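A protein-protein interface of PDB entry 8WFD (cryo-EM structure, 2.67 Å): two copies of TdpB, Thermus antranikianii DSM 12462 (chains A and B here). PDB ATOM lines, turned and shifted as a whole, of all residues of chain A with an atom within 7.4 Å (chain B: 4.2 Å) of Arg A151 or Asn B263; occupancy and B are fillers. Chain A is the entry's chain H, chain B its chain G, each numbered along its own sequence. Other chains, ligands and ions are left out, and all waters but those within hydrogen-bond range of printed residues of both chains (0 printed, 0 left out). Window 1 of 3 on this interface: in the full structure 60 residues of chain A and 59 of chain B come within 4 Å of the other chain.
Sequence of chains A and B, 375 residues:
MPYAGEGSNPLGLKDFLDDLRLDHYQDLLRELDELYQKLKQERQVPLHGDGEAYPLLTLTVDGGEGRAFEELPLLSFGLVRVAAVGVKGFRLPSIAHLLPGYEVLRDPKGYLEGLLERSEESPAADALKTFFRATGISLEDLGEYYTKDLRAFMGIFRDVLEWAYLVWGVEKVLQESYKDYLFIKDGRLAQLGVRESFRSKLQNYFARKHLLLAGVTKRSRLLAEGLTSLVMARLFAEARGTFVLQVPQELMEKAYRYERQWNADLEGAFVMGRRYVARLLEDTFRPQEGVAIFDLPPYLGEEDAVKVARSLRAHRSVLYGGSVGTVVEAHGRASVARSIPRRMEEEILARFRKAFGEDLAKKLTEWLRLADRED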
ATOM      1  N   PHE A  69     -19.776  10.223 -28.066  1.00  0.00           N
ATOM      2  CA  PHE A  69     -20.761  10.976 -27.297  1.00  0.00           C
ATOM      3  C   PHE A  69     -20.163  11.527 -26.010  1.00  0.00           C
ATOM      4  O   PHE A  69     -20.538  12.621 -25.574  1.00  0.00           O
ATOM      5  CB  PHE A  69     -21.977  10.103 -26.986  1.00  0.00           C
ATOM      6  CG  PHE A  69     -23.144  10.871 -26.434  1.00  0.00           C
ATOM      7  CD1 PHE A  69     -23.691  11.928 -27.141  1.00  0.00           C
ATOM      8  CD2 PHE A  69     -23.693  10.537 -25.209  1.00  0.00           C
ATOM      9  CE1 PHE A  69     -24.765  12.637 -26.635  1.00  0.00           C
ATOM     10  CE2 PHE A  69     -24.766  11.242 -24.699  1.00  0.00           C
ATOM     11  CZ  PHE A  69     -25.302  12.293 -25.413  1.00  0.00           C
ATOM     12  N   GLU A  70     -19.238  10.794 -25.390  1.00  0.00           N
ATOM     13  CA  GLU A  70     -18.574  11.300 -24.194  1.00  0.00           C
ATOM     14  C   GLU A  70     -17.502  12.323 -24.549  1.00  0.00           C
ATOM     15  O   GLU A  70     -17.511  13.447 -24.034  1.00  0.00           O
ATOM     16  CB  GLU A  70     -17.967  10.141 -23.399  1.00  0.00           C
ATOM     17  CG  GLU A  70     -17.573  10.498 -21.971  1.00  0.00           C
ATOM     18  CD  GLU A  70     -16.233  11.206 -21.891  1.00  0.00           C
ATOM     19  OE1 GLU A  70     -15.412  11.041 -22.818  1.00  0.00           O
ATOM     20  OE2 GLU A  70     -15.998  11.929 -20.900  1.00  0.00           O
ATOM     21  N   LEU A 105     -29.603  19.692 -25.959  1.00  0.00           N
ATOM     22  CA  LEU A 105     -29.080  18.939 -24.826  1.00  0.00           C
ATOM     23  C   LEU A 105     -28.002  19.729 -24.096  1.00  0.00           C
ATOM     24  O   LEU A 105     -27.906  19.669 -22.865  1.00  0.00           O
ATOM     25  CB  LEU A 105     -28.531  17.594 -25.299  1.00  0.00           C
ATOM     26  CG  LEU A 105     -29.542  16.458 -25.459  1.00  0.00           C
ATOM     27  CD1 LEU A 105     -30.518  16.770 -26.581  1.00  0.00           C
ATOM     28  CD2 LEU A 105     -28.827  15.139 -25.716  1.00  0.00           C
ATOM     29  N   ARG A 106     -27.179  20.472 -24.839  1.00  0.00           N
ATOM     30  CA  ARG A 106     -26.148  21.285 -24.206  1.00  0.00           C
ATOM     31  C   ARG A 106     -26.758  22.382 -23.343  1.00  0.00           C
ATOM     32  O   ARG A 106     -26.145  22.809 -22.358  1.00  0.00           O
ATOM     33  CB  ARG A 106     -25.235  21.891 -25.271  1.00  0.00           C
ATOM     34  CG  ARG A 106     -24.587  20.860 -26.180  1.00  0.00           C
ATOM     35  CD  ARG A 106     -23.767  19.871 -25.381  1.00  0.00           C
ATOM     36  NE  ARG A 106     -22.676  20.523 -24.672  1.00  0.00           N
ATOM     37  CZ  ARG A 106     -22.094  20.035 -23.585  1.00  0.00           C
ATOM     38  NH1 ARG A 106     -22.485  18.893 -23.046  1.00  0.00           N
ATOM     39  NH2 ARG A 106     -21.099  20.712 -23.025  1.00  0.00           N
ATOM     40  N   PRO A 108     -30.183  22.498 -21.609  1.00  0.00           N
ATOM     41  CA  PRO A 108     -31.486  21.901 -21.289  1.00  0.00           C
ATOM     42  C   PRO A 108     -32.507  22.918 -20.806  1.00  0.00           C
ATOM     43  O   PRO A 108     -32.214  24.114 -20.710  1.00  0.00           O
ATOM     44  CB  PRO A 108     -31.146  20.889 -20.186  1.00  0.00           C
ATOM     45  CG  PRO A 108     -29.693  20.606 -20.356  1.00  0.00           C
ATOM     46  CD  PRO A 108     -29.089  21.889 -20.836  1.00  0.00           C
ATOM     47  N   TYR A 145     -32.622  19.780 -11.311  1.00  0.00           N
ATOM     48  CA  TYR A 145     -31.569  18.773 -11.382  1.00  0.00           C
ATOM     49  C   TYR A 145     -31.335  18.318 -12.818  1.00  0.00           C
ATOM     50  O   TYR A 145     -30.188  18.114 -13.231  1.00  0.00           O
ATOM     51  CB  TYR A 145     -31.918  17.581 -10.492  1.00  0.00           C
ATOM     52  CG  TYR A 145     -30.963  16.417 -10.624  1.00  0.00           C
ATOM     53  CD1 TYR A 145     -29.714  16.447 -10.018  1.00  0.00           C
ATOM     54  CD2 TYR A 145     -31.309  15.289 -11.354  1.00  0.00           C
ATOM     55  CE1 TYR A 145     -28.838  15.386 -10.136  1.00  0.00           C
ATOM     56  CE2 TYR A 145     -30.440  14.223 -11.477  1.00  0.00           C
ATOM     57  CZ  TYR A 145     -29.206  14.277 -10.865  1.00  0.00           C
ATOM     58  OH  TYR A 145     -28.337  13.216 -10.986  1.00  0.00           O
ATOM     59  N   TYR A 146     -32.409  18.148 -13.593  1.00  0.00           N
ATOM     60  CA  TYR A 146     -32.261  17.721 -14.978  1.00  0.00           C
ATOM     61  C   TYR A 146     -31.655  18.808 -15.854  1.00  0.00           C
ATOM     62  O   TYR A 146     -31.111  18.498 -16.918  1.00  0.00           O
ATOM     63  CB  TYR A 146     -33.612  17.282 -15.546  1.00  0.00           C
ATOM     64  CG  TYR A 146     -34.509  18.422 -15.968  1.00  0.00           C
ATOM     65  CD1 TYR A 146     -35.032  19.304 -15.033  1.00  0.00           C
ATOM     66  CD2 TYR A 146     -34.834  18.615 -17.302  1.00  0.00           C
ATOM     67  CE1 TYR A 146     -35.853  20.346 -15.416  1.00  0.00           C
ATOM     68  CE2 TYR A 146     -35.654  19.655 -17.695  1.00  0.00           C
ATOM     69  CZ  TYR A 146     -36.160  20.517 -16.748  1.00  0.00           C
ATOM     70  OH  TYR A 146     -36.976  21.554 -17.133  1.00  0.00           O
ATOM     71  N   LYS A 148     -29.162  20.588 -14.781  1.00  0.00           N
ATOM     72  CA  LYS A 148     -27.792  20.753 -14.305  1.00  0.00           C
ATOM     73  C   LYS A 148     -26.788  20.569 -15.435  1.00  0.00           C
ATOM     74  O   LYS A 148     -25.880  21.388 -15.613  1.00  0.00           O
ATOM     75  CB  LYS A 148     -27.520  19.763 -13.172  1.00  0.00           C
ATOM     76  CG  LYS A 148     -26.102  19.787 -12.633  1.00  0.00           C
ATOM     77  CD  LYS A 148     -25.920  18.725 -11.563  1.00  0.00           C
ATOM     78  CE  LYS A 148     -24.474  18.630 -11.112  1.00  0.00           C
ATOM     79  NZ  LYS A 148     -24.261  17.484 -10.186  1.00  0.00           N
ATOM     80  N   ASP A 149     -26.934  19.500 -16.211  1.00  0.00           N
ATOM     81  CA  ASP A 149     -26.042  19.230 -17.335  1.00  0.00           C
ATOM     82  C   ASP A 149     -26.572  18.013 -18.086  1.00  0.00           C
ATOM     83  O   ASP A 149     -27.559  17.388 -17.685  1.00  0.00           O
ATOM     84  CB  ASP A 149     -24.598  19.029 -16.870  1.00  0.00           C
ATOM     85  CG  ASP A 149     -24.488  18.071 -15.706  1.00  0.00           C
ATOM     86  OD1 ASP A 149     -25.505  17.438 -15.355  1.00  0.00           O
ATOM     87  OD2 ASP A 149     -23.384  17.952 -15.137  1.00  0.00           O
ATOM     88  N   LEU A 150     -25.893  17.678 -19.188  1.00  0.00           N
ATOM     89  CA  LEU A 150     -26.387  16.642 -20.090  1.00  0.00           C
ATOM     90  C   LEU A 150     -26.365  15.262 -19.440  1.00  0.00           C
ATOM     91  O   LEU A 150     -27.245  14.433 -19.706  1.00  0.00           O
ATOM     92  CB  LEU A 150     -25.565  16.642 -21.379  1.00  0.00           C
ATOM     93  CG  LEU A 150     -26.144  15.841 -22.546  1.00  0.00           C
ATOM     94  CD1 LEU A 150     -27.644  16.050 -22.639  1.00  0.00           C
ATOM     95  CD2 LEU A 150     -25.463  16.227 -23.851  1.00  0.00           C
ATOM     96  N   ARG A 151     -25.366  14.989 -18.600  1.00  0.00           N
ATOM     97  CA  ARG A 151     -25.289  13.679 -17.963  1.00  0.00           C
ATOM     98  C   ARG A 151     -26.502  13.424 -17.079  1.00  0.00           C
ATOM     99  O   ARG A 151     -27.059  12.319 -17.077  1.00  0.00           O
ATOM    100  CB  ARG A 151     -23.998  13.559 -17.154  1.00  0.00           C
ATOM    101  CG  ARG A 151     -22.741  13.501 -18.004  1.00  0.00           C
ATOM    102  CD  ARG A 151     -21.502  13.318 -17.147  1.00  0.00           C
ATOM    103  NE  ARG A 151     -21.541  12.060 -16.411  1.00  0.00           N
ATOM    104  CZ  ARG A 151     -20.730  11.754 -15.408  1.00  0.00           C
ATOM    105  NH1 ARG A 151     -19.795  12.593 -14.993  1.00  0.00           N
ATOM    106  NH2 ARG A 151     -20.860  10.574 -14.807  1.00  0.00           N
ATOM    107  N   ALA A 152     -26.924  14.433 -16.314  1.00  0.00           N
ATOM    108  CA  ALA A 152     -28.136  14.297 -15.514  1.00  0.00           C
ATOM    109  C   ALA A 152     -29.380  14.313 -16.392  1.00  0.00           C
ATOM    110  O   ALA A 152     -30.363  13.616 -16.102  1.00  0.00           O
ATOM    111  CB  ALA A 152     -28.202  15.410 -14.469  1.00  0.00           C
ATOM    112  N   PHE A 153     -29.361  15.115 -17.459  1.00  0.00           N
ATOM    113  CA  PHE A 153     -30.530  15.219 -18.324  1.00  0.00           C
ATOM    114  C   PHE A 153     -30.863  13.882 -18.966  1.00  0.00           C
ATOM    115  O   PHE A 153     -32.036  13.510 -19.061  1.00  0.00           O
ATOM    116  CB  PHE A 153     -30.307  16.283 -19.398  1.00  0.00           C
ATOM    117  CG  PHE A 153     -31.426  16.373 -20.396  1.00  0.00           C
ATOM    118  CD1 PHE A 153     -32.545  17.144 -20.135  1.00  0.00           C
ATOM    119  CD2 PHE A 153     -31.361  15.680 -21.593  1.00  0.00           C
ATOM    120  CE1 PHE A 153     -33.578  17.223 -21.050  1.00  0.00           C
ATOM    121  CE2 PHE A 153     -32.390  15.756 -22.510  1.00  0.00           C
ATOM    122  CZ  PHE A 153     -33.499  16.528 -22.239  1.00  0.00           C
ATOM    123  N   MET A 154     -29.849  13.148 -19.426  1.00  0.00           N
ATOM    124  CA  MET A 154     -30.107  11.863 -20.070  1.00  0.00           C
ATOM    125  C   MET A 154     -30.843  10.916 -19.127  1.00  0.00           C
ATOM    126  O   MET A 154     -31.880  10.342 -19.481  1.00  0.00           O
ATOM    127  CB  MET A 154     -28.794  11.240 -20.544  1.00  0.00           C
ATOM    128  CG  MET A 154     -27.931  12.164 -21.389  1.00  0.00           C
ATOM    129  SD  MET A 154     -28.766  12.774 -22.867  1.00  0.00           S
ATOM    130  CE  MET A 154     -28.449  11.437 -24.012  1.00  0.00           C
ATOM    131  N   GLY A 155     -30.322  10.752 -17.909  1.00  0.00           N
ATOM    132  CA  GLY A 155     -30.949   9.846 -16.963  1.00  0.00           C
ATOM    133  C   GLY A 155     -32.336  10.294 -16.545  1.00  0.00           C
ATOM    134  O   GLY A 155     -33.260   9.477 -16.455  1.00  0.00           O
ATOM    135  N   ILE A 156     -32.506  11.592 -16.278  1.00  0.00           N
ATOM    136  CA  ILE A 156     -33.816  12.082 -15.869  1.00  0.00           C
ATOM    137  C   ILE A 156     -34.826  11.897 -16.994  1.00  0.00           C
ATOM    138  O   ILE A 156     -35.978  11.514 -16.757  1.00  0.00           O
ATOM    139  CB  ILE A 156     -33.723  13.552 -15.421  1.00  0.00           C
ATOM    140  CG1 ILE A 156     -33.087  13.641 -14.033  1.00  0.00           C
ATOM    141  CG2 ILE A 156     -35.098  14.196 -15.422  1.00  0.00           C
ATOM    142  CD1 ILE A 156     -33.795  12.811 -12.984  1.00  0.00           C
ATOM    143  N   GLU B 259     -17.243  22.174 -21.944  1.00  0.00           N
ATOM    144  CA  GLU B 259     -16.920  21.208 -20.901  1.00  0.00           C
ATOM    145  C   GLU B 259     -17.723  21.464 -19.631  1.00  0.00           C
ATOM    146  O   GLU B 259     -18.128  20.511 -18.957  1.00  0.00           O
ATOM    147  CB  GLU B 259     -15.417  21.210 -20.614  1.00  0.00           C
ATOM    148  CG  GLU B 259     -14.924  22.336 -19.733  1.00  0.00           C
ATOM    149  CD  GLU B 259     -13.511  22.089 -19.240  1.00  0.00           C
ATOM    150  OE1 GLU B 259     -12.897  21.095 -19.680  1.00  0.00           O
ATOM    151  OE2 GLU B 259     -13.015  22.884 -18.414  1.00  0.00           O
ATOM    152  N   ARG B 260     -17.974  22.731 -19.292  1.00  0.00           N
ATOM    153  CA  ARG B 260     -18.826  23.025 -18.145  1.00  0.00           C
ATOM    154  C   ARG B 260     -20.239  22.509 -18.365  1.00  0.00           C
ATOM    155  O   ARG B 260     -20.835  21.900 -17.469  1.00  0.00           O
ATOM    156  CB  ARG B 260     -18.851  24.527 -17.871  1.00  0.00           C
ATOM    157  CG  ARG B 260     -19.995  24.951 -16.962  1.00  0.00           C
ATOM    158  CD  ARG B 260     -20.110  26.463 -16.858  1.00  0.00           C
ATOM    159  NE  ARG B 260     -18.949  27.062 -16.213  1.00  0.00           N
ATOM    160  CZ  ARG B 260     -18.182  27.992 -16.765  1.00  0.00           C
ATOM    161  NH1 ARG B 260     -18.427  28.457 -17.979  1.00  0.00           N
ATOM    162  NH2 ARG B 260     -17.145  28.467 -16.082  1.00  0.00           N
ATOM    163  N   GLN B 261     -20.798  22.745 -19.554  1.00  0.00           N
ATOM    164  CA  GLN B 261     -22.150  22.277 -19.834  1.00  0.00           C
ATOM    165  C   GLN B 261     -22.243  20.759 -19.825  1.00  0.00           C
ATOM    166  O   GLN B 261     -23.275  20.217 -19.416  1.00  0.00           O
ATOM    167  CB  GLN B 261     -22.636  22.827 -21.175  1.00  0.00           C
ATOM    168  CG  GLN B 261     -22.496  24.332 -21.309  1.00  0.00           C
ATOM    169  CD  GLN B 261     -23.112  24.862 -22.586  1.00  0.00           C
ATOM    170  OE1 GLN B 261     -22.754  24.438 -23.684  1.00  0.00           O
ATOM    171  NE2 GLN B 261     -24.044  25.798 -22.449  1.00  0.00           N
ATOM    172  N   TRP B 262     -21.195  20.063 -20.263  1.00  0.00           N
ATOM    173  CA  TRP B 262     -21.187  18.608 -20.203  1.00  0.00           C
ATOM    174  C   TRP B 262     -20.949  18.072 -18.798  1.00  0.00           C
ATOM    175  O   TRP B 262     -21.397  16.962 -18.490  1.00  0.00           O
ATOM    176  CB  TRP B 262     -20.126  18.042 -21.154  1.00  0.00           C
ATOM    177  CG  TRP B 262     -19.741  16.628 -20.848  1.00  0.00           C
ATOM    178  CD1 TRP B 262     -18.575  16.201 -20.283  1.00  0.00           C
ATOM    179  CD2 TRP B 262     -20.529  15.454 -21.078  1.00  0.00           C
ATOM    180  NE1 TRP B 262     -18.586  14.834 -20.152  1.00  0.00           N
ATOM    181  CE2 TRP B 262     -19.774  14.351 -20.631  1.00  0.00           C
ATOM    182  CE3 TRP B 262     -21.798  15.227 -21.619  1.00  0.00           C
ATOM    183  CZ2 TRP B 262     -20.246  13.042 -20.711  1.00  0.00           C
ATOM    184  CZ3 TRP B 262     -22.264  13.927 -21.697  1.00  0.00           C
ATOM    185  CH2 TRP B 262     -21.489  12.851 -21.245  1.00  0.00           C
ATOM    186  N   ASN B 263     -20.266  18.830 -17.938  1.00  0.00           N
ATOM    187  CA  ASN B 263     -20.001  18.390 -16.568  1.00  0.00           C
ATOM    188  C   ASN B 263     -19.861  19.637 -15.698  1.00  0.00           C
ATOM    189  O   ASN B 263     -18.864  20.357 -15.798  1.00  0.00           O
ATOM    190  CB  ASN B 263     -18.755  17.519 -16.501  1.00  0.00           C
ATOM    191  CG  ASN B 263     -18.664  16.730 -15.212  1.00  0.00           C
ATOM    192  OD1 ASN B 263     -19.527  16.842 -14.342  1.00  0.00           O
ATOM    193  ND2 ASN B 263     -17.616  15.925 -15.083  1.00  0.00           N
ATOM    194  N   ALA B 264     -20.862  19.879 -14.847  1.00  0.00           N
ATOM    195  CA  ALA B 264     -20.839  21.064 -13.996  1.00  0.00           C
ATOM    196  C   ALA B 264     -19.670  21.037 -13.020  1.00  0.00           C
ATOM    197  O   ALA B 264     -19.108  22.090 -12.696  1.00  0.00           O
ATOM    198  CB  ALA B 264     -22.160  21.194 -13.237  1.00  0.00           C
ATOM    199  N   ASP B 265     -19.283  19.851 -12.550  1.00  0.00           N
ATOM    200  CA  ASP B 265     -18.182  19.752 -11.601  1.00  0.00           C
ATOM    201  C   ASP B 265     -16.861  20.233 -12.185  1.00  0.00           C
ATOM    202  O   ASP B 265     -15.924  20.490 -11.420  1.00  0.00           O
ATOM    203  CB  ASP B 265     -18.039  18.310 -11.112  1.00  0.00           C
ATOM    204  CG  ASP B 265     -19.343  17.742 -10.591  1.00  0.00           C
ATOM    205  OD1 ASP B 265     -20.231  18.540 -10.221  1.00  0.00           O
ATOM    206  OD2 ASP B 265     -19.481  16.502 -10.549  1.00  0.00           O
ATOM    207  N   LEU B 266     -16.766  20.368 -13.505  1.00  0.00           N
ATOM    208  CA  LEU B 266     -15.568  20.901 -14.136  1.00  0.00           C
ATOM    209  C   LEU B 266     -15.468  22.416 -14.025  1.00  0.00           C
ATOM    210  O   LEU B 266     -14.447  22.981 -14.431  1.00  0.00           O
ATOM    211  CB  LEU B 266     -15.517  20.485 -15.608  1.00  0.00           C
ATOM    212  CG  LEU B 266     -15.355  18.985 -15.858  1.00  0.00           C
ATOM    213  CD1 LEU B 266     -14.918  18.717 -17.291  1.00  0.00           C
ATOM    214  CD2 LEU B 266     -14.374  18.377 -14.867  1.00  0.00           C
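No position is printed for both chains.
Printed residues of chain B within 4 Å of Arg A151: Trp B262 (3.5 Å) and Asn B263 (3.98 Å).
Of the printed residues of chain A, Asn B263 touches Asp A149 (3.7 Å) and Arg A151 (3.98 Å).
Of the printed residues of chain B, Asp A149 touches Gln B261, Asn B263 and Ala B264.
Printed residues of chain A within 4 Å of Gln B261: Arg A106 (3.2 Å), Asp A149 (3.1 Å) and Leu A150 (3.7 Å).
Of the printed residues of chain B, Glu A70 touches Trp B262.
Of the printed residues of chain B, Leu A150 touches Gln B261 (3.7 Å).
Ile A156 touches none of the printed residues of chain B.
The nearest printed residue of chain A that does not touch Gln B261 is Lys A148 (4.8 Å).
Hydrophobic or aromatic side chains of chain B that line the printed part of chain A: Trp B262 and Ala B264.
Among the printed residues, 9 pairs touch across the chains.
Among the printed residues, no Asp or Glu carboxylate lies within 4 Å of a Lys or Arg side-chain nitrogen of the other chain.
OD2 of Asp A149 lies within hydrogen-bond range of N of Ala B264 (3.2 Å).
N of Trp B262 lies close to NH2 of Arg A106, at 2.8 Å.
OD1 of Asp A149 lies within hydrogen-bond range of N of Ala A152 (3.5 Å).
Among the printed residues, merely in contact across the chains: Asp A149 with Gln B261, Arg A106 with Gln B261, Arg A151 with Trp B262, Leu A150 with Gln B261, Asp A149 with Asn B263, Glu A70 with Trp B262 and Arg A151 with Asn B263.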
